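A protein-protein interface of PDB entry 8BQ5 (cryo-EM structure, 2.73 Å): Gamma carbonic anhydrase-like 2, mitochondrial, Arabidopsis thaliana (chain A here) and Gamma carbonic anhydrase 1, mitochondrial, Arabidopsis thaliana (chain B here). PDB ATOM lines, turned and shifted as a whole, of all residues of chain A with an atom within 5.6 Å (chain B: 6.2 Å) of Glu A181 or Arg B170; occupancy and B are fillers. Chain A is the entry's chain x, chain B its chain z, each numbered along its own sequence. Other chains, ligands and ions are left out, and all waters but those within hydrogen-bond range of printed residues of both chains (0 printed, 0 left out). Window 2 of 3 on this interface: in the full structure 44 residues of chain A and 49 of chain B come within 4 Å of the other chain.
The backbone NH of Glu A181 sits at hydrogen-bond distance from the backbone carbonyl oxygen of Trp A198 (2.8 Å).
O of Leu B168 lies within hydrogen-bond range of N of Ala B186, at 3.0 Å.
O of Arg B170 is in hydrogen-bond range of OG1 of Thr B173, at 2.9 Å.
The backbone carbonyl oxygen (O) of Glu A181 is in hydrogen-bond range of the side-chain hydroxyl (OG) of Ser A184, at 2.6 Å.
O of Glu A181 is in hydrogen-bond range of OG of Ser A166, 3.2 Å away.
The backbone carbonyl oxygen (O) of Gln A164 is in hydrogen-bond range of the backbone NH (N) of Gly A183, at 2.9 Å.
The side-chain carboxylate of Glu A181 is in salt-bridge range of the guanidinium group of Arg B170, at 2.9 Å.
The side-chain amide nitrogen (ND2) of Asn B184 is in hydrogen-bond range of the backbone carbonyl oxygen (O) of Gly A183 (3.5 Å).
Ile A179 touches none of the printed residues of chain B.
Glu A181 touches just one residue of chain B: Arg B170 (2.9 Å).
Of the printed residues of chain B, Ala A182 touches Leu B168.
Of the printed residues of chain B, Gly A183 touches Leu B168 and Asn B184.
Thr B150 touches none of the printed residues of chain A.
Of the printed residues of chain A, Arg B170 touches Glu A181.
Printed residues of chain A within 4 Å of Asn B184: Gly A183 (3.5 Å).
The nearest residue of chain B that does not touch Glu A181 is Leu B168 (5.9 Å).
The nearest printed residue of chain A that does not touch Leu B168 is Ser A184 (5.2 Å).
Printed residues of chain B that touch a printed residue of chain A: Leu B168, Arg B170 and Asn B184.
Hydrophobic or aromatic side chains of chain B within 4 Å of the printed part of chain A: Leu B168.
Among the printed residues, 4 pairs touch across the chains.
Among the printed residues, Asp or Glu carboxylates within 4 Å of a Lys or Arg side-chain nitrogen of the other chain: Glu A181 with Arg B170 (2.9 Å).
Ala A182 touches Leu B168.
Gly A183 touches Leu B168 (CA to CD1, 3.3 Å).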
ATOM      1  N   ILE A 162      24.144  20.905  15.971  1.00  0.00           N
ATOM      2  CA  ILE A 162      25.126  19.842  16.140  1.00  0.00           C
ATOM      3  C   ILE A 162      24.726  18.697  15.222  1.00  0.00           C
ATOM      4  O   ILE A 162      23.609  18.177  15.316  1.00  0.00           O
ATOM      5  CB  ILE A 162      25.209  19.379  17.601  1.00  0.00           C
ATOM      6  CG1 ILE A 162      25.450  20.570  18.533  1.00  0.00           C
ATOM      7  CG2 ILE A 162      26.302  18.337  17.764  1.00  0.00           C
ATOM      8  CD1 ILE A 162      26.756  21.291  18.292  1.00  0.00           C
ATOM      9  N   GLY A 163      25.633  18.303  14.331  1.00  0.00           N
ATOM     10  CA  GLY A 163      25.328  17.242  13.397  1.00  0.00           C
ATOM     11  C   GLY A 163      25.159  15.900  14.081  1.00  0.00           C
ATOM     12  O   GLY A 163      25.606  15.674  15.205  1.00  0.00           O
ATOM     13  N   GLN A 164      24.458  15.006  13.385  1.00  0.00           N
ATOM     14  CA  GLN A 164      24.185  13.654  13.933  1.00  0.00           C
ATOM     15  C   GLN A 164      25.478  12.894  14.180  1.00  0.00           C
ATOM     16  O   GLN A 164      26.387  13.012  13.362  1.00  0.00           O
ATOM     17  CB  GLN A 164      23.332  12.806  12.987  1.00  0.00           C
ATOM     18  CG  GLN A 164      21.958  13.381  12.692  1.00  0.00           C
ATOM     19  CD  GLN A 164      21.283  12.615  11.581  1.00  0.00           C
ATOM     20  OE1 GLN A 164      21.020  11.422  11.698  1.00  0.00           O
ATOM     21  NE2 GLN A 164      21.004  13.298  10.484  1.00  0.00           N
ATOM     22  N   SER A 166      27.746  13.285  16.574  1.00  0.00           N
ATOM     23  CA  SER A 166      28.869  14.124  16.959  1.00  0.00           C
ATOM     24  C   SER A 166      29.248  13.873  18.413  1.00  0.00           C
ATOM     25  O   SER A 166      28.460  13.356  19.208  1.00  0.00           O
ATOM     26  CB  SER A 166      28.536  15.601  16.750  1.00  0.00           C
ATOM     27  OG  SER A 166      28.514  15.929  15.372  1.00  0.00           O
ATOM     28  N   ILE A 179      27.681  25.742  13.180  1.00  0.00           N
ATOM     29  CA  ILE A 179      27.131  24.460  12.765  1.00  0.00           C
ATOM     30  C   ILE A 179      28.255  23.434  12.748  1.00  0.00           C
ATOM     31  O   ILE A 179      29.334  23.697  12.206  1.00  0.00           O
ATOM     32  CB  ILE A 179      26.447  24.548  11.387  1.00  0.00           C
ATOM     33  CG1 ILE A 179      25.245  25.492  11.454  1.00  0.00           C
ATOM     34  CG2 ILE A 179      26.004  23.175  10.919  1.00  0.00           C
ATOM     35  CD1 ILE A 179      24.726  25.915  10.103  1.00  0.00           C
ATOM     36  N   LEU A 180      28.008  22.281  13.358  1.00  0.00           N
ATOM     37  CA  LEU A 180      28.926  21.153  13.335  1.00  0.00           C
ATOM     38  C   LEU A 180      28.373  20.100  12.390  1.00  0.00           C
ATOM     39  O   LEU A 180      27.179  19.785  12.438  1.00  0.00           O
ATOM     40  CB  LEU A 180      29.110  20.560  14.732  1.00  0.00           C
ATOM     41  CG  LEU A 180      30.318  21.026  15.537  1.00  0.00           C
ATOM     42  CD1 LEU A 180      30.234  20.470  16.946  1.00  0.00           C
ATOM     43  CD2 LEU A 180      31.612  20.602  14.866  1.00  0.00           C
ATOM     44  N   GLU A 181      29.249  19.566  11.554  1.00  0.00           N
ATOM     45  CA  GLU A 181      28.792  18.549  10.587  1.00  0.00           C
ATOM     46  C   GLU A 181      28.569  17.223  11.302  1.00  0.00           C
ATOM     47  O   GLU A 181      29.068  17.043  12.419  1.00  0.00           O
ATOM     48  CB  GLU A 181      29.803  18.358   9.463  1.00  0.00           C
ATOM     49  CG  GLU A 181      29.637  19.363   8.344  1.00  0.00           C
ATOM     50  CD  GLU A 181      30.436  19.031   7.099  1.00  0.00           C
ATOM     51  OE1 GLU A 181      31.314  18.147   7.179  1.00  0.00           O
ATOM     52  OE2 GLU A 181      30.180  19.656   6.056  1.00  0.00           O
ATOM     53  N   ALA A 182      27.835  16.329  10.664  1.00  0.00           N
ATOM     54  CA  ALA A 182      27.614  15.002  11.216  1.00  0.00           C
ATOM     55  C   ALA A 182      28.936  14.256  11.342  1.00  0.00           C
ATOM     56  O   ALA A 182      29.825  14.384  10.495  1.00  0.00           O
ATOM     57  CB  ALA A 182      26.641  14.216  10.340  1.00  0.00           C
ATOM     58  N   GLY A 183      29.069  13.485  12.418  1.00  0.00           N
ATOM     59  CA  GLY A 183      30.272  12.717  12.657  1.00  0.00           C
ATOM     60  C   GLY A 183      31.441  13.493  13.218  1.00  0.00           C
ATOM     61  O   GLY A 183      32.557  12.963  13.245  1.00  0.00           O
ATOM     62  N   SER A 184      31.228  14.725  13.665  1.00  0.00           N
ATOM     63  CA  SER A 184      32.313  15.560  14.158  1.00  0.00           C
ATOM     64  C   SER A 184      32.738  15.144  15.562  1.00  0.00           C
ATOM     65  O   SER A 184      31.922  14.713  16.379  1.00  0.00           O
ATOM     66  CB  SER A 184      31.892  17.028  14.165  1.00  0.00           C
ATOM     67  OG  SER A 184      31.572  17.471  12.860  1.00  0.00           O
ATOM     68  N   LEU A 197      31.297  26.925   9.900  1.00  0.00           N
ATOM     69  CA  LEU A 197      30.918  25.531   9.726  1.00  0.00           C
ATOM     70  C   LEU A 197      32.146  24.660   9.949  1.00  0.00           C
ATOM     71  O   LEU A 197      33.196  24.894   9.344  1.00  0.00           O
ATOM     72  CB  LEU A 197      30.329  25.284   8.335  1.00  0.00           C
ATOM     73  CG  LEU A 197      30.095  23.821   7.958  1.00  0.00           C
ATOM     74  CD1 LEU A 197      28.919  23.263   8.733  1.00  0.00           C
ATOM     75  CD2 LEU A 197      29.859  23.673   6.467  1.00  0.00           C
ATOM     76  N   TRP A 198      32.021  23.709  10.869  1.00  0.00           N
ATOM     77  CA  TRP A 198      33.160  22.826  11.217  1.00  0.00           C
ATOM     78  C   TRP A 198      32.711  21.375  11.093  1.00  0.00           C
ATOM     79  O   TRP A 198      31.507  21.119  11.158  1.00  0.00           O
ATOM     80  CB  TRP A 198      33.656  23.128  12.633  1.00  0.00           C
ATOM     81  CG  TRP A 198      34.635  24.248  12.775  1.00  0.00           C
ATOM     82  CD1 TRP A 198      34.470  25.532  12.353  1.00  0.00           C
ATOM     83  CD2 TRP A 198      35.915  24.202  13.431  1.00  0.00           C
ATOM     84  NE1 TRP A 198      35.569  26.272  12.676  1.00  0.00           N
ATOM     85  CE2 TRP A 198      36.470  25.494  13.342  1.00  0.00           C
ATOM     86  CE3 TRP A 198      36.652  23.207  14.076  1.00  0.00           C
ATOM     87  CZ2 TRP A 198      37.723  25.811  13.860  1.00  0.00           C
ATOM     88  CZ3 TRP A 198      37.889  23.519  14.595  1.00  0.00           C
ATOM     89  CH2 TRP A 198      38.415  24.805  14.489  1.00  0.00           C
ATOM     90  N   GLY A 199      33.648  20.461  10.899  1.00  0.00           N
ATOM     91  CA  GLY A 199      33.355  19.042  10.804  1.00  0.00           C
ATOM     92  C   GLY A 199      34.637  18.242  10.784  1.00  0.00           C
ATOM     93  O   GLY A 199      35.740  18.790  10.692  1.00  0.00           O
ATOM     94  N   GLY A 200      34.475  16.930  10.878  1.00  0.00           N
ATOM     95  CA  GLY A 200      35.580  15.997  10.819  1.00  0.00           C
ATOM     96  C   GLY A 200      35.929  15.425  12.184  1.00  0.00           C
ATOM     97  O   GLY A 200      35.406  15.829  13.222  1.00  0.00           O
ATOM     98  N   ILE A 206      35.775  24.279   8.082  1.00  0.00           N
ATOM     99  CA  ILE A 206      35.362  24.051   6.702  1.00  0.00           C
ATOM    100  C   ILE A 206      35.189  25.369   5.960  1.00  0.00           C
ATOM    101  O   ILE A 206      35.865  25.624   4.962  1.00  0.00           O
ATOM    102  CB  ILE A 206      34.079  23.196   6.634  1.00  0.00           C
ATOM    103  CG1 ILE A 206      34.340  21.817   7.234  1.00  0.00           C
ATOM    104  CG2 ILE A 206      33.584  23.086   5.200  1.00  0.00           C
ATOM    105  CD1 ILE A 206      33.168  20.900   7.157  1.00  0.00           C
ATOM    106  N   THR B 150      27.176   5.877   9.423  1.00  0.00           N
ATOM    107  CA  THR B 150      26.151   6.904   9.290  1.00  0.00           C
ATOM    108  C   THR B 150      25.890   7.172   7.816  1.00  0.00           C
ATOM    109  O   THR B 150      26.804   7.546   7.076  1.00  0.00           O
ATOM    110  CB  THR B 150      26.558   8.201   9.991  1.00  0.00           C
ATOM    111  OG1 THR B 150      26.921   7.920  11.348  1.00  0.00           O
ATOM    112  CG2 THR B 150      25.406   9.197   9.976  1.00  0.00           C
ATOM    113  N   LEU B 151      24.643   6.982   7.400  1.00  0.00           N
ATOM    114  CA  LEU B 151      24.212   7.237   6.033  1.00  0.00           C
ATOM    115  C   LEU B 151      23.239   8.405   6.058  1.00  0.00           C
ATOM    116  O   LEU B 151      22.160   8.303   6.650  1.00  0.00           O
ATOM    117  CB  LEU B 151      23.558   5.998   5.415  1.00  0.00           C
ATOM    118  CG  LEU B 151      24.366   4.766   4.978  1.00  0.00           C
ATOM    119  CD1 LEU B 151      25.506   4.382   5.915  1.00  0.00           C
ATOM    120  CD2 LEU B 151      23.423   3.590   4.806  1.00  0.00           C
ATOM    121  N   LEU B 152      23.649   9.497   5.413  1.00  0.00           N
ATOM    122  CA  LEU B 152      22.820  10.718   5.445  1.00  0.00           C
ATOM    123  C   LEU B 152      21.734  10.641   4.378  1.00  0.00           C
ATOM    124  O   LEU B 152      21.559   9.571   3.779  1.00  0.00           O
ATOM    125  CB  LEU B 152      23.737  11.937   5.314  1.00  0.00           C
ATOM    126  CG  LEU B 152      24.703  12.114   6.486  1.00  0.00           C
ATOM    127  CD1 LEU B 152      25.541  13.372   6.333  1.00  0.00           C
ATOM    128  CD2 LEU B 152      23.948  12.136   7.807  1.00  0.00           C
ATOM    129  N   ASP B 153      21.007  11.732   4.163  1.00  0.00           N
ATOM    130  CA  ASP B 153      19.850  11.673   3.282  1.00  0.00           C
ATOM    131  C   ASP B 153      20.269  11.677   1.814  1.00  0.00           C
ATOM    132  O   ASP B 153      21.292  12.250   1.431  1.00  0.00           O
ATOM    133  CB  ASP B 153      18.860  12.803   3.609  1.00  0.00           C
ATOM    134  CG  ASP B 153      19.336  14.182   3.177  1.00  0.00           C
ATOM    135  OD1 ASP B 153      20.476  14.335   2.705  1.00  0.00           O
ATOM    136  OD2 ASP B 153      18.547  15.139   3.321  1.00  0.00           O
ATOM    137  N   GLY B 154      19.483  10.981   0.995  1.00  0.00           N
ATOM    138  CA  GLY B 154      19.771  10.853  -0.415  1.00  0.00           C
ATOM    139  C   GLY B 154      20.805   9.809  -0.767  1.00  0.00           C
ATOM    140  O   GLY B 154      21.091   9.622  -1.956  1.00  0.00           O
ATOM    141  N   VAL B 155      21.329   9.107   0.234  1.00  0.00           N
ATOM    142  CA  VAL B 155      22.372   8.074  -0.015  1.00  0.00           C
ATOM    143  C   VAL B 155      21.724   6.843  -0.650  1.00  0.00           C
ATOM    144  O   VAL B 155      20.654   6.442  -0.182  1.00  0.00           O
ATOM    145  CB  VAL B 155      23.122   7.711   1.284  1.00  0.00           C
ATOM    146  CG1 VAL B 155      23.919   6.422   1.160  1.00  0.00           C
ATOM    147  CG2 VAL B 155      24.001   8.844   1.771  1.00  0.00           C
ATOM    148  N   LEU B 168      31.219   7.476   7.523  1.00  0.00           N
ATOM    149  CA  LEU B 168      30.202   8.556   7.410  1.00  0.00           C
ATOM    150  C   LEU B 168      29.939   8.775   5.917  1.00  0.00           C
ATOM    151  O   LEU B 168      30.753   9.454   5.274  1.00  0.00           O
ATOM    152  CB  LEU B 168      30.740   9.829   8.075  1.00  0.00           C
ATOM    153  CG  LEU B 168      29.785  11.017   8.241  1.00  0.00           C
ATOM    154  CD1 LEU B 168      30.077  11.815   9.502  1.00  0.00           C
ATOM    155  CD2 LEU B 168      29.757  11.922   7.024  1.00  0.00           C
ATOM    156  N   VAL B 169      28.867   8.193   5.388  1.00  0.00           N
ATOM    157  CA  VAL B 169      28.495   8.382   3.956  1.00  0.00           C
ATOM    158  C   VAL B 169      27.762   9.717   3.845  1.00  0.00           C
ATOM    159  O   VAL B 169      26.650   9.822   4.387  1.00  0.00           O
ATOM    160  CB  VAL B 169      27.642   7.215   3.423  1.00  0.00           C
ATOM    161  CG1 VAL B 169      27.422   7.303   1.927  1.00  0.00           C
ATOM    162  CG2 VAL B 169      28.244   5.869   3.788  1.00  0.00           C
ATOM    163  N   ARG B 170      28.358  10.684   3.153  1.00  0.00           N
ATOM    164  CA  ARG B 170      27.766  12.045   3.046  1.00  0.00           C
ATOM    165  C   ARG B 170      26.474  12.008   2.233  1.00  0.00           C
ATOM    166  O   ARG B 170      26.204  10.988   1.599  1.00  0.00           O
ATOM    167  CB  ARG B 170      28.798  13.006   2.453  1.00  0.00           C
ATOM    168  CG  ARG B 170      29.939  13.323   3.408  1.00  0.00           C
ATOM    169  CD  ARG B 170      30.899  14.391   2.929  1.00  0.00           C
ATOM    170  NE  ARG B 170      30.340  15.734   2.946  1.00  0.00           N
ATOM    171  CZ  ARG B 170      30.315  16.532   4.008  1.00  0.00           C
ATOM    172  NH1 ARG B 170      30.812  16.118   5.161  1.00  0.00           N
ATOM    173  NH2 ARG B 170      29.790  17.740   3.912  1.00  0.00           N
ATOM    174  N   GLN B 171      25.726  13.108   2.232  1.00  0.00           N
ATOM    175  CA  GLN B 171      24.420  13.168   1.530  1.00  0.00           C
ATOM    176  C   GLN B 171      24.556  12.850   0.041  1.00  0.00           C
ATOM    177  O   GLN B 171      25.585  13.232  -0.544  1.00  0.00           O
ATOM    178  CB  GLN B 171      23.820  14.567   1.673  1.00  0.00           C
ATOM    179  CG  GLN B 171      23.772  15.052   3.116  1.00  0.00           C
ATOM    180  CD  GLN B 171      22.993  16.331   3.307  1.00  0.00           C
ATOM    181  OE1 GLN B 171      22.203  16.741   2.460  1.00  0.00           O
ATOM    182  NE2 GLN B 171      23.204  16.973   4.444  1.00  0.00           N
ATOM    183  N   ASN B 172      23.561  12.167  -0.533  1.00  0.00           N
ATOM    184  CA  ASN B 172      23.529  11.912  -2.000  1.00  0.00           C
ATOM    185  C   ASN B 172      24.777  11.165  -2.461  1.00  0.00           C
ATOM    186  O   ASN B 172      25.239  11.437  -3.582  1.00  0.00           O
ATOM    187  CB  ASN B 172      23.347  13.223  -2.773  1.00  0.00           C
ATOM    188  CG  ASN B 172      22.072  13.953  -2.407  1.00  0.00           C
ATOM    189  OD1 ASN B 172      20.987  13.382  -2.466  1.00  0.00           O
ATOM    190  ND2 ASN B 172      22.195  15.214  -2.032  1.00  0.00           N
ATOM    191  N   THR B 173      25.277  10.241  -1.637  1.00  0.00           N
ATOM    192  CA  THR B 173      26.470   9.452  -2.023  1.00  0.00           C
ATOM    193  C   THR B 173      25.999   8.070  -2.463  1.00  0.00           C
ATOM    194  O   THR B 173      25.461   7.331  -1.626  1.00  0.00           O
ATOM    195  CB  THR B 173      27.545   9.458  -0.935  1.00  0.00           C
ATOM    196  OG1 THR B 173      27.935  10.815  -0.732  1.00  0.00           O
ATOM    197  CG2 THR B 173      28.753   8.623  -1.298  1.00  0.00           C
ATOM    198  N   ASN B 184      35.746   8.724   6.971  1.00  0.00           N
ATOM    199  CA  ASN B 184      34.987   9.957   7.184  1.00  0.00           C
ATOM    200  C   ASN B 184      35.641  11.088   6.402  1.00  0.00           C
ATOM    201  O   ASN B 184      36.665  11.640   6.847  1.00  0.00           O
ATOM    202  CB  ASN B 184      34.924  10.293   8.675  1.00  0.00           C
ATOM    203  CG  ASN B 184      33.929  11.393   8.990  1.00  0.00           C
ATOM    204  OD1 ASN B 184      33.323  11.979   8.094  1.00  0.00           O
ATOM    205  ND2 ASN B 184      33.752  11.673  10.275  1.00  0.00           N
ATOM    206  N   PRO B 185      35.118  11.503   5.211  1.00  0.00           N
ATOM    207  CA  PRO B 185      33.918  10.915   4.603  1.00  0.00           C
ATOM    208  C   PRO B 185      34.191   9.584   3.900  1.00  0.00           C
ATOM    209  O   PRO B 185      35.331   9.298   3.599  1.00  0.00           O
ATOM    210  CB  PRO B 185      33.495  11.933   3.540  1.00  0.00           C
ATOM    211  CG  PRO B 185      34.796  12.543   3.094  1.00  0.00           C
ATOM    212  CD  PRO B 185      35.632  12.594   4.356  1.00  0.00           C
ATOM    213  N   ALA B 186      33.139   8.812   3.639  1.00  0.00           N
ATOM    214  CA  ALA B 186      33.332   7.498   3.043  1.00  0.00           C
ATOM    215  C   ALA B 186      33.832   7.629   1.610  1.00  0.00           C
ATOM    216  O   ALA B 186      33.275   8.388   0.813  1.00  0.00           O
ATOM    217  CB  ALA B 186      32.028   6.703   3.080  1.00  0.00           C
